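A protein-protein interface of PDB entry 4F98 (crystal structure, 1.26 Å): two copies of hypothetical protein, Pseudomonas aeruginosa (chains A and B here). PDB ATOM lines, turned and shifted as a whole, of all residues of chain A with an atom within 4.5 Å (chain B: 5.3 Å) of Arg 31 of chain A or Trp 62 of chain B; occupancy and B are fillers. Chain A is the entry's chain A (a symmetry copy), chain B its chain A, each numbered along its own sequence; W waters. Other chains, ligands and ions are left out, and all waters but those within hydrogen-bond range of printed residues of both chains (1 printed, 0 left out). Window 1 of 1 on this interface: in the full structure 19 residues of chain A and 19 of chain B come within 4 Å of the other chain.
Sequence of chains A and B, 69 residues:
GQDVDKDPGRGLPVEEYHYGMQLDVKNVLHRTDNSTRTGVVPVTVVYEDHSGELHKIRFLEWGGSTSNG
The guanidinium group (NH2) of Arg 31 of chain A is in hydrogen-bond range of the backbone carbonyl oxygen (O) of Trp 62 of chain B (2.9 Å).
The indole nitrogen (NE1) of Trp 62 of chain B sits at hydrogen-bond distance from the side-chain hydroxyl (OH) of Tyr 17 of chain A (3.1 Å).
O of Gly 63 of chain B lies within hydrogen-bond range of NE of Arg 31 of chain A.
The backbone carbonyl oxygen (O) of Val 43 of chain A sits at hydrogen-bond distance from the backbone NH (N) of Phe 59 of chain A, at 2.9 Å.
OE1 of Glu 61 of chain A lies within salt-bridge range of NH2 of Arg 31 of chain A, 2.8 Å away.
The backbone carbonyl oxygen (O) of Ile 57 of chain A sits at hydrogen-bond distance from the backbone NH (N) of Val 45 of chain A, 2.9 Å away.
The backbone NH of Gly 63 of chain B lies within hydrogen-bond range of the backbone carbonyl oxygen of Gly 39 of chain B.
Among the printed residues, merely in contact across the chains: Val 28 of chain A with Thr 66 of chain B (3.2 Å), Phe 59 of chain A with Trp 62 of chain B (3.4 Å), Arg 31 of chain A with Gly 64 of chain B (3.5 Å), Val 25 of chain A with Trp 62 of chain B (3.7 Å), Ile 57 of chain A with Trp 62 of chain B (3.8 Å), His 30 of chain A with Thr 66 of chain B (3.8 Å), Arg 31 of chain A with Thr 66 of chain B (3.8 Å), Leu 23 of chain A with Trp 62 of chain B (3.8 Å), Val 45 of chain A with Trp 62 of chain B (3.9 Å), Val 28 of chain A with Trp 62 of chain B (3.9 Å) and Val 28 of chain A with Gly 39 of chain B (3.9 Å).
Of chain B, only Trp 62, Gly 63, Gly 64 and Thr 66 come within 4 Å of Arg 31 of chain A.
Printed residues of chain A within 4 Å of Trp 62 of chain B: Tyr 17, Leu 23, Val 25, Val 28, Arg 31, Val 45, Ile 57 and Phe 59.
Printed residues of chain A within 4 Å of Thr 66 of chain B: Val 28 (3.2 Å), His 30 (3.8 Å) and Arg 31 (3.8 Å).
Printed residues of chain B within 4 Å of Val 28 of chain A: Gly 39, Trp 62 and Thr 66.
Of the printed residues of chain B, Phe 59 of chain A touches Trp 62 (3.4 Å).
Printed residues of chain B within 4 Å of His 30 of chain A: Thr 66.
The nearest residue of chain B that does not touch Arg 31 of chain A is Ser 65 of chain B (4.4 Å).
The nearest printed residue of chain A that does not touch Trp 62 of chain B is Tyr 47 of chain A (4.1 Å).
The nearest printed residue of chain B that does not touch Val 28 of chain A is Ser 65 of chain B (4.2 Å).
Of the 10 printed residues of chain B, 5 touch a printed residue of chain A.
Along chain B the printed residues that touch a printed residue of chain A span positions 39 to 66.
Among the printed residues, no Asp or Glu carboxylate lies within 4 Å of a Lys or Arg side-chain nitrogen of the other chain.
1 position is printed for both chains.
Of the 14 pairs that touch across the chains among the printed residues, none has its exchanged pair printed and touching as well.
Water W1 bridges the side-chain carboxylate of Glu 61 of chain A and the backbone NH of Trp 62 of chain B.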
ATOM      1  N   TYR A  17      14.380   8.187  16.808  1.00  0.00           N
ATOM      2  CA  TYR A  17      13.531   9.138  17.498  1.00  0.00           C
ATOM      3  C   TYR A  17      12.272   8.397  18.000  1.00  0.00           C
ATOM      4  O   TYR A  17      11.870   7.329  17.515  1.00  0.00           O
ATOM      5  CB  TYR A  17      13.336  10.429  16.652  1.00  0.00           C
ATOM      6  CG  TYR A  17      12.414  11.484  17.224  1.00  0.00           C
ATOM      7  CD1 TYR A  17      12.699  12.128  18.425  1.00  0.00           C
ATOM      8  CD2 TYR A  17      11.246  11.812  16.578  1.00  0.00           C
ATOM      9  CE1 TYR A  17      11.843  13.061  18.959  1.00  0.00           C
ATOM     10  CE2 TYR A  17      10.387  12.767  17.106  1.00  0.00           C
ATOM     11  CZ  TYR A  17      10.694  13.377  18.299  1.00  0.00           C
ATOM     12  OH  TYR A  17       9.870  14.333  18.848  1.00  0.00           O
ATOM     13  N   LEU A  23      14.055  15.984  24.275  1.00  0.00           N
ATOM     14  CA  LEU A  23      15.280  16.250  23.505  1.00  0.00           C
ATOM     15  C   LEU A  23      15.900  17.544  24.002  1.00  0.00           C
ATOM     16  O   LEU A  23      15.229  18.371  24.635  1.00  0.00           O
ATOM     17  CB  LEU A  23      14.985  16.350  22.001  1.00  0.00           C
ATOM     18  CG  LEU A  23      14.441  15.102  21.306  1.00  0.00           C
ATOM     19  CD1 LEU A  23      14.175  15.394  19.830  1.00  0.00           C
ATOM     20  CD2 LEU A  23      15.380  13.935  21.434  1.00  0.00           C
ATOM     21  N   VAL A  25      16.827  20.623  22.544  1.00  0.00           N
ATOM     22  CA  VAL A  25      16.633  21.450  21.354  1.00  0.00           C
ATOM     23  C   VAL A  25      16.974  22.898  21.662  1.00  0.00           C
ATOM     24  O   VAL A  25      16.247  23.575  22.386  1.00  0.00           O
ATOM     25  CB  VAL A  25      15.176  21.352  20.822  1.00  0.00           C
ATOM     26  CG1 VAL A  25      15.007  22.226  19.568  1.00  0.00           C
ATOM     27  CG2 VAL A  25      14.788  19.884  20.541  1.00  0.00           C
ATOM     28  N   VAL A  28      15.884  24.913  15.934  1.00  0.00           N
ATOM     29  CA  VAL A  28      15.357  24.102  14.844  1.00  0.00           C
ATOM     30  C   VAL A  28      15.879  24.745  13.559  1.00  0.00           C
ATOM     31  O   VAL A  28      15.566  25.898  13.247  1.00  0.00           O
ATOM     32  CB  VAL A  28      13.810  24.040  14.871  1.00  0.00           C
ATOM     33  CG1 VAL A  28      13.278  23.237  13.677  1.00  0.00           C
ATOM     34  CG2 VAL A  28      13.310  23.462  16.203  1.00  0.00           C
ATOM     35  N   HIS A  30      15.813  23.101  10.318  1.00  0.00           N
ATOM     36  CA  HIS A  30      15.023  22.695   9.170  1.00  0.00           C
ATOM     37  C   HIS A  30      13.813  21.937   9.654  1.00  0.00           C
ATOM     38  O   HIS A  30      13.905  21.138  10.579  1.00  0.00           O
ATOM     39  CB  HIS A  30      15.821  21.759   8.242  1.00  0.00           C
ATOM     40  CG  HIS A  30      14.985  21.157   7.158  1.00  0.00           C
ATOM     41  ND1 HIS A  30      14.525  19.865   7.207  1.00  0.00           N
ATOM     42  CD2 HIS A  30      14.453  21.699   6.041  1.00  0.00           C
ATOM     43  CE1 HIS A  30      13.763  19.633   6.155  1.00  0.00           C
ATOM     44  NE2 HIS A  30      13.706  20.730   5.425  1.00  0.00           N
ATOM     45  N   ARG A  31      12.680  22.178   9.013  1.00  0.00           N
ATOM     46  CA  ARG A  31      11.520  21.304   9.151  1.00  0.00           C
ATOM     47  C   ARG A  31      10.753  21.310   7.845  1.00  0.00           C
ATOM     48  O   ARG A  31      10.626  22.343   7.190  1.00  0.00           O
ATOM     49  CB  ARG A  31      10.664  21.715  10.362  1.00  0.00           C
ATOM     50  CG  ARG A  31      10.006  23.100  10.310  1.00  0.00           C
ATOM     51  CD  ARG A  31       8.567  23.011   9.939  1.00  0.00           C
ATOM     52  NE  ARG A  31       7.738  22.415  10.994  1.00  0.00           N
ATOM     53  CZ  ARG A  31       6.989  21.309  10.914  1.00  0.00           C
ATOM     54  NH1 ARG A  31       6.873  20.607   9.788  1.00  0.00           N
ATOM     55  NH2 ARG A  31       6.304  20.919  11.983  1.00  0.00           N
ATOM     56  N   THR A  32      10.250  20.152   7.436  1.00  0.00           N
ATOM     57  CA  THR A  32       9.462  20.003   6.210  1.00  0.00           C
ATOM     58  C   THR A  32       8.320  21.017   6.187  1.00  0.00           C
ATOM     59  O   THR A  32       7.649  21.222   7.194  1.00  0.00           O
ATOM     60  CB  THR A  32       8.854  18.598   6.130  1.00  0.00           C
ATOM     61  OG1 THR A  32       9.918  17.647   6.326  1.00  0.00           O
ATOM     62  CG2 THR A  32       8.137  18.388   4.785  1.00  0.00           C
ATOM     63  N   ASP A  33       8.105  21.657   5.049  1.00  0.00           N
ATOM     64  CA  ASP A  33       6.947  22.551   4.932  1.00  0.00           C
ATOM     65  C   ASP A  33       5.727  21.680   4.586  1.00  0.00           C
ATOM     66  O   ASP A  33       5.511  21.275   3.436  1.00  0.00           O
ATOM     67  CB  ASP A  33       7.140  23.706   3.939  1.00  0.00           C
ATOM     68  CG  ASP A  33       6.084  24.814   4.122  1.00  0.00           C
ATOM     69  OD1 ASP A  33       5.089  24.582   4.850  1.00  0.00           O
ATOM     70  OD2 ASP A  33       6.217  25.911   3.527  1.00  0.00           O
ATOM     71  N   ASN A  34       4.929  21.416   5.618  1.00  0.00           N
ATOM     72  CA  ASN A  34       3.683  20.647   5.493  1.00  0.00           C
ATOM     73  C   ASN A  34       2.441  21.526   5.639  1.00  0.00           C
ATOM     74  O   ASN A  34       1.342  21.022   5.855  1.00  0.00           O
ATOM     75  CB  ASN A  34       3.669  19.478   6.493  1.00  0.00           C
ATOM     76  CG  ASN A  34       4.567  18.347   6.075  1.00  0.00           C
ATOM     77  OD1 ASN A  34       4.650  18.041   4.882  1.00  0.00           O
ATOM     78  ND2 ASN A  34       5.213  17.704   7.041  1.00  0.00           N
ATOM     79  N   VAL A  43       7.476  14.070   8.175  1.00  0.00           N
ATOM     80  CA  VAL A  43       8.207  15.288   8.491  1.00  0.00           C
ATOM     81  C   VAL A  43       9.634  14.933   8.873  1.00  0.00           C
ATOM     82  O   VAL A  43       9.882  13.946   9.579  1.00  0.00           O
ATOM     83  CB  VAL A  43       7.503  16.087   9.635  1.00  0.00           C
ATOM     84  CG1 VAL A  43       7.221  15.225  10.855  1.00  0.00           C
ATOM     85  CG2 VAL A  43       8.298  17.341  10.009  1.00  0.00           C
ATOM     86  N   THR A  44      10.560  15.743   8.370  1.00  0.00           N
ATOM     87  CA  THR A  44      11.955  15.679   8.743  1.00  0.00           C
ATOM     88  C   THR A  44      12.327  16.965   9.450  1.00  0.00           C
ATOM     89  O   THR A  44      11.981  18.049   8.980  1.00  0.00           O
ATOM     90  CB  THR A  44      12.832  15.483   7.520  1.00  0.00           C
ATOM     91  OG1 THR A  44      12.410  14.284   6.864  1.00  0.00           O
ATOM     92  CG2 THR A  44      14.308  15.380   7.904  1.00  0.00           C
ATOM     93  N   VAL A  45      13.014  16.837  10.569  1.00  0.00           N
ATOM     94  CA  VAL A  45      13.541  17.943  11.345  1.00  0.00           C
ATOM     95  C   VAL A  45      15.056  17.818  11.471  1.00  0.00           C
ATOM     96  O   VAL A  45      15.566  16.728  11.701  1.00  0.00           O
ATOM     97  CB  VAL A  45      12.887  18.022  12.745  1.00  0.00           C
ATOM     98  CG1 VAL A  45      13.626  19.027  13.657  1.00  0.00           C
ATOM     99  CG2 VAL A  45      11.404  18.370  12.617  1.00  0.00           C
ATOM    100  N   TYR A  47      17.721  19.698  13.968  1.00  0.00           N
ATOM    101  CA  TYR A  47      17.847  20.598  15.112  1.00  0.00           C
ATOM    102  C   TYR A  47      19.279  20.592  15.652  1.00  0.00           C
ATOM    103  O   TYR A  47      20.034  19.645  15.453  1.00  0.00           O
ATOM    104  CB  TYR A  47      16.781  20.284  16.201  1.00  0.00           C
ATOM    105  CG  TYR A  47      17.040  19.065  17.030  1.00  0.00           C
ATOM    106  CD1 TYR A  47      17.823  19.137  18.182  1.00  0.00           C
ATOM    107  CD2 TYR A  47      16.521  17.829  16.655  1.00  0.00           C
ATOM    108  CE1 TYR A  47      18.086  18.004  18.935  1.00  0.00           C
ATOM    109  CE2 TYR A  47      16.780  16.678  17.424  1.00  0.00           C
ATOM    110  CZ  TYR A  47      17.572  16.772  18.545  1.00  0.00           C
ATOM    111  OH  TYR A  47      17.848  15.664  19.298  1.00  0.00           O
ATOM    112  N   ILE A  57      16.065  13.903  12.316  1.00  0.00           N
ATOM    113  CA  ILE A  57      15.030  12.937  12.723  1.00  0.00           C
ATOM    114  C   ILE A  57      13.899  12.984  11.699  1.00  0.00           C
ATOM    115  O   ILE A  57      13.652  14.028  11.088  1.00  0.00           O
ATOM    116  CB  ILE A  57      14.535  13.191  14.155  1.00  0.00           C
ATOM    117  CG1 ILE A  57      14.097  14.647  14.345  1.00  0.00           C
ATOM    118  CG2 ILE A  57      15.639  12.812  15.168  1.00  0.00           C
ATOM    119  CD1 ILE A  57      13.367  14.931  15.658  1.00  0.00           C
ATOM    120  N   PHE A  59       9.811  11.437  11.051  1.00  0.00           N
ATOM    121  CA  PHE A  59       8.687  10.895  11.805  1.00  0.00           C
ATOM    122  C   PHE A  59       7.395  11.351  11.111  1.00  0.00           C
ATOM    123  O   PHE A  59       7.444  11.731   9.930  1.00  0.00           O
ATOM    124  CB  PHE A  59       8.817  11.297  13.304  1.00  0.00           C
ATOM    125  CG  PHE A  59       8.980  12.780  13.536  1.00  0.00           C
ATOM    126  CD1 PHE A  59      10.212  13.397  13.390  1.00  0.00           C
ATOM    127  CD2 PHE A  59       7.911  13.551  13.948  1.00  0.00           C
ATOM    128  CE1 PHE A  59      10.361  14.762  13.577  1.00  0.00           C
ATOM    129  CE2 PHE A  59       8.054  14.917  14.160  1.00  0.00           C
ATOM    130  CZ  PHE A  59       9.302  15.524  13.979  1.00  0.00           C
ATOM    131  N   GLU A  61       3.581  13.610  11.347  1.00  0.00           N
ATOM    132  CA  GLU A  61       2.835  14.685  11.984  1.00  0.00           C
ATOM    133  C   GLU A  61       1.550  14.939  11.221  1.00  0.00           C
ATOM    134  O   GLU A  61       1.365  14.434  10.112  1.00  0.00           O
ATOM    135  CB  GLU A  61       3.683  15.944  12.043  1.00  0.00           C
ATOM    136  CG  GLU A  61       3.883  16.624  10.692  1.00  0.00           C
ATOM    137  CD  GLU A  61       4.677  17.924  10.775  1.00  0.00           C
ATOM    138  OE1 GLU A  61       5.143  18.320  11.871  1.00  0.00           O
ATOM    139  OE2 GLU A  61       4.859  18.581   9.726  1.00  0.00           O
ATOM    140  N   GLY B  39       9.890  24.287  17.953  1.00  0.00           N
ATOM    141  CA  GLY B  39      10.071  23.202  18.899  1.00  0.00           C
ATOM    142  C   GLY B  39       8.739  22.545  19.235  1.00  0.00           C
ATOM    143  O   GLY B  39       7.722  22.800  18.587  1.00  0.00           O
ATOM    144  N   VAL B  40       8.735  21.724  20.277  1.00  0.00           N
ATOM    145  CA  VAL B  40       7.587  20.905  20.593  1.00  0.00           C
ATOM    146  C   VAL B  40       6.547  21.719  21.349  1.00  0.00           C
ATOM    147  O   VAL B  40       6.844  22.391  22.345  1.00  0.00           O
ATOM    148  CB  VAL B  40       7.999  19.614  21.311  1.00  0.00           C
ATOM    149  CG1 VAL B  40       6.788  18.868  21.799  1.00  0.00           C
ATOM    150  CG2 VAL B  40       8.846  18.747  20.383  1.00  0.00           C
ATOM    151  N   VAL B  41       5.309  21.605  20.870  1.00  0.00           N
ATOM    152  CA  VAL B  41       4.184  22.395  21.348  1.00  0.00           C
ATOM    153  C   VAL B  41       2.923  21.535  21.343  1.00  0.00           C
ATOM    154  O   VAL B  41       2.837  20.563  20.601  1.00  0.00           O
ATOM    155  CB  VAL B  41       3.986  23.682  20.476  1.00  0.00           C
ATOM    156  CG1 VAL B  41       5.190  24.650  20.584  1.00  0.00           C
ATOM    157  CG2 VAL B  41       3.669  23.329  19.015  1.00  0.00           C
ATOM    158  N   LEU B  60       1.201  16.328  21.094  1.00  0.00           N
ATOM    159  CA  LEU B  60       2.335  17.226  20.882  1.00  0.00           C
ATOM    160  C   LEU B  60       2.803  17.133  19.449  1.00  0.00           C
ATOM    161  O   LEU B  60       2.706  16.077  18.812  1.00  0.00           O
ATOM    162  CB  LEU B  60       3.510  16.828  21.784  1.00  0.00           C
ATOM    163  CG  LEU B  60       3.252  16.889  23.284  1.00  0.00           C
ATOM    164  CD1 LEU B  60       4.417  16.203  24.012  1.00  0.00           C
ATOM    165  CD2 LEU B  60       3.029  18.339  23.750  1.00  0.00           C
ATOM    166  N   GLU B  61       3.324  18.250  18.941  1.00  0.00           N
ATOM    167  CA  GLU B  61       3.921  18.294  17.615  1.00  0.00           C
ATOM    168  C   GLU B  61       5.037  19.321  17.590  1.00  0.00           C
ATOM    169  O   GLU B  61       5.184  20.115  18.521  1.00  0.00           O
ATOM    170  CB  GLU B  61       2.863  18.626  16.578  1.00  0.00           C
ATOM    171  CG  GLU B  61       2.381  20.072  16.619  1.00  0.00           C
ATOM    172  CD  GLU B  61       1.370  20.411  15.528  1.00  0.00           C
ATOM    173  OE1 GLU B  61       0.968  19.528  14.732  1.00  0.00           O
ATOM    174  OE2 GLU B  61       0.945  21.585  15.450  1.00  0.00           O
ATOM    175  N   TRP B  62       5.797  19.320  16.514  1.00  0.00           N
ATOM    176  CA  TRP B  62       6.792  20.360  16.301  1.00  0.00           C
ATOM    177  C   TRP B  62       6.116  21.563  15.629  1.00  0.00           C
ATOM    178  O   TRP B  62       5.313  21.402  14.712  1.00  0.00           O
ATOM    179  CB  TRP B  62       7.927  19.850  15.448  1.00  0.00           C
ATOM    180  CG  TRP B  62       8.754  18.828  16.143  1.00  0.00           C
ATOM    181  CD1 TRP B  62       8.386  17.562  16.490  1.00  0.00           C
ATOM    182  CD2 TRP B  62      10.098  18.995  16.634  1.00  0.00           C
ATOM    183  NE1 TRP B  62       9.415  16.916  17.111  1.00  0.00           N
ATOM    184  CE2 TRP B  62      10.473  17.771  17.227  1.00  0.00           C
ATOM    185  CE3 TRP B  62      11.021  20.048  16.610  1.00  0.00           C
ATOM    186  CZ2 TRP B  62      11.733  17.571  17.802  1.00  0.00           C
ATOM    187  CZ3 TRP B  62      12.279  19.847  17.188  1.00  0.00           C
ATOM    188  CH2 TRP B  62      12.614  18.617  17.772  1.00  0.00           C
ATOM    189  N   GLY B  63       6.426  22.750  16.119  1.00  0.00           N
ATOM    190  CA  GLY B  63       5.882  23.971  15.559  1.00  0.00           C
ATOM    191  C   GLY B  63       6.288  24.176  14.114  1.00  0.00           C
ATOM    192  O   GLY B  63       7.224  23.551  13.611  1.00  0.00           O
ATOM    193  N   GLY B  64       5.569  25.062  13.451  1.00  0.00           N
ATOM    194  CA  GLY B  64       5.745  25.288  12.042  1.00  0.00           C
ATOM    195  C   GLY B  64       6.935  26.120  11.627  1.00  0.00           C
ATOM    196  O   GLY B  64       7.182  26.218  10.438  1.00  0.00           O
ATOM    197  N   SER B  65       7.673  26.690  12.581  1.00  0.00           N
ATOM    198  CA  SER B  65       8.797  27.574  12.284  1.00  0.00           C
ATOM    199  C   SER B  65      10.150  26.970  12.653  1.00  0.00           C
ATOM    200  O   SER B  65      10.255  26.101  13.496  1.00  0.00           O
ATOM    201  CB  SER B  65       8.618  28.900  13.013  1.00  0.00           C
ATOM    202  OG  SER B  65       7.572  29.658  12.421  1.00  0.00           O
ATOM    203  N   THR B  66      11.188  27.456  11.978  1.00  0.00           N
ATOM    204  CA  THR B  66      12.571  27.232  12.359  1.00  0.00           C
ATOM    205  C   THR B  66      13.040  28.447  13.169  1.00  0.00           C
ATOM    206  O   THR B  66      12.328  29.462  13.259  1.00  0.00           O
ATOM    207  CB  THR B  66      13.450  27.006  11.103  1.00  0.00           C
ATOM    208  OG1 THR B  66      13.247  28.086  10.205  1.00  0.00           O
ATOM    209  CG2 THR B  66      13.056  25.743  10.365  1.00  0.00           C
HETATM  210  O   HOH W   1       5.485  17.437  14.461  1.00  0.00           O
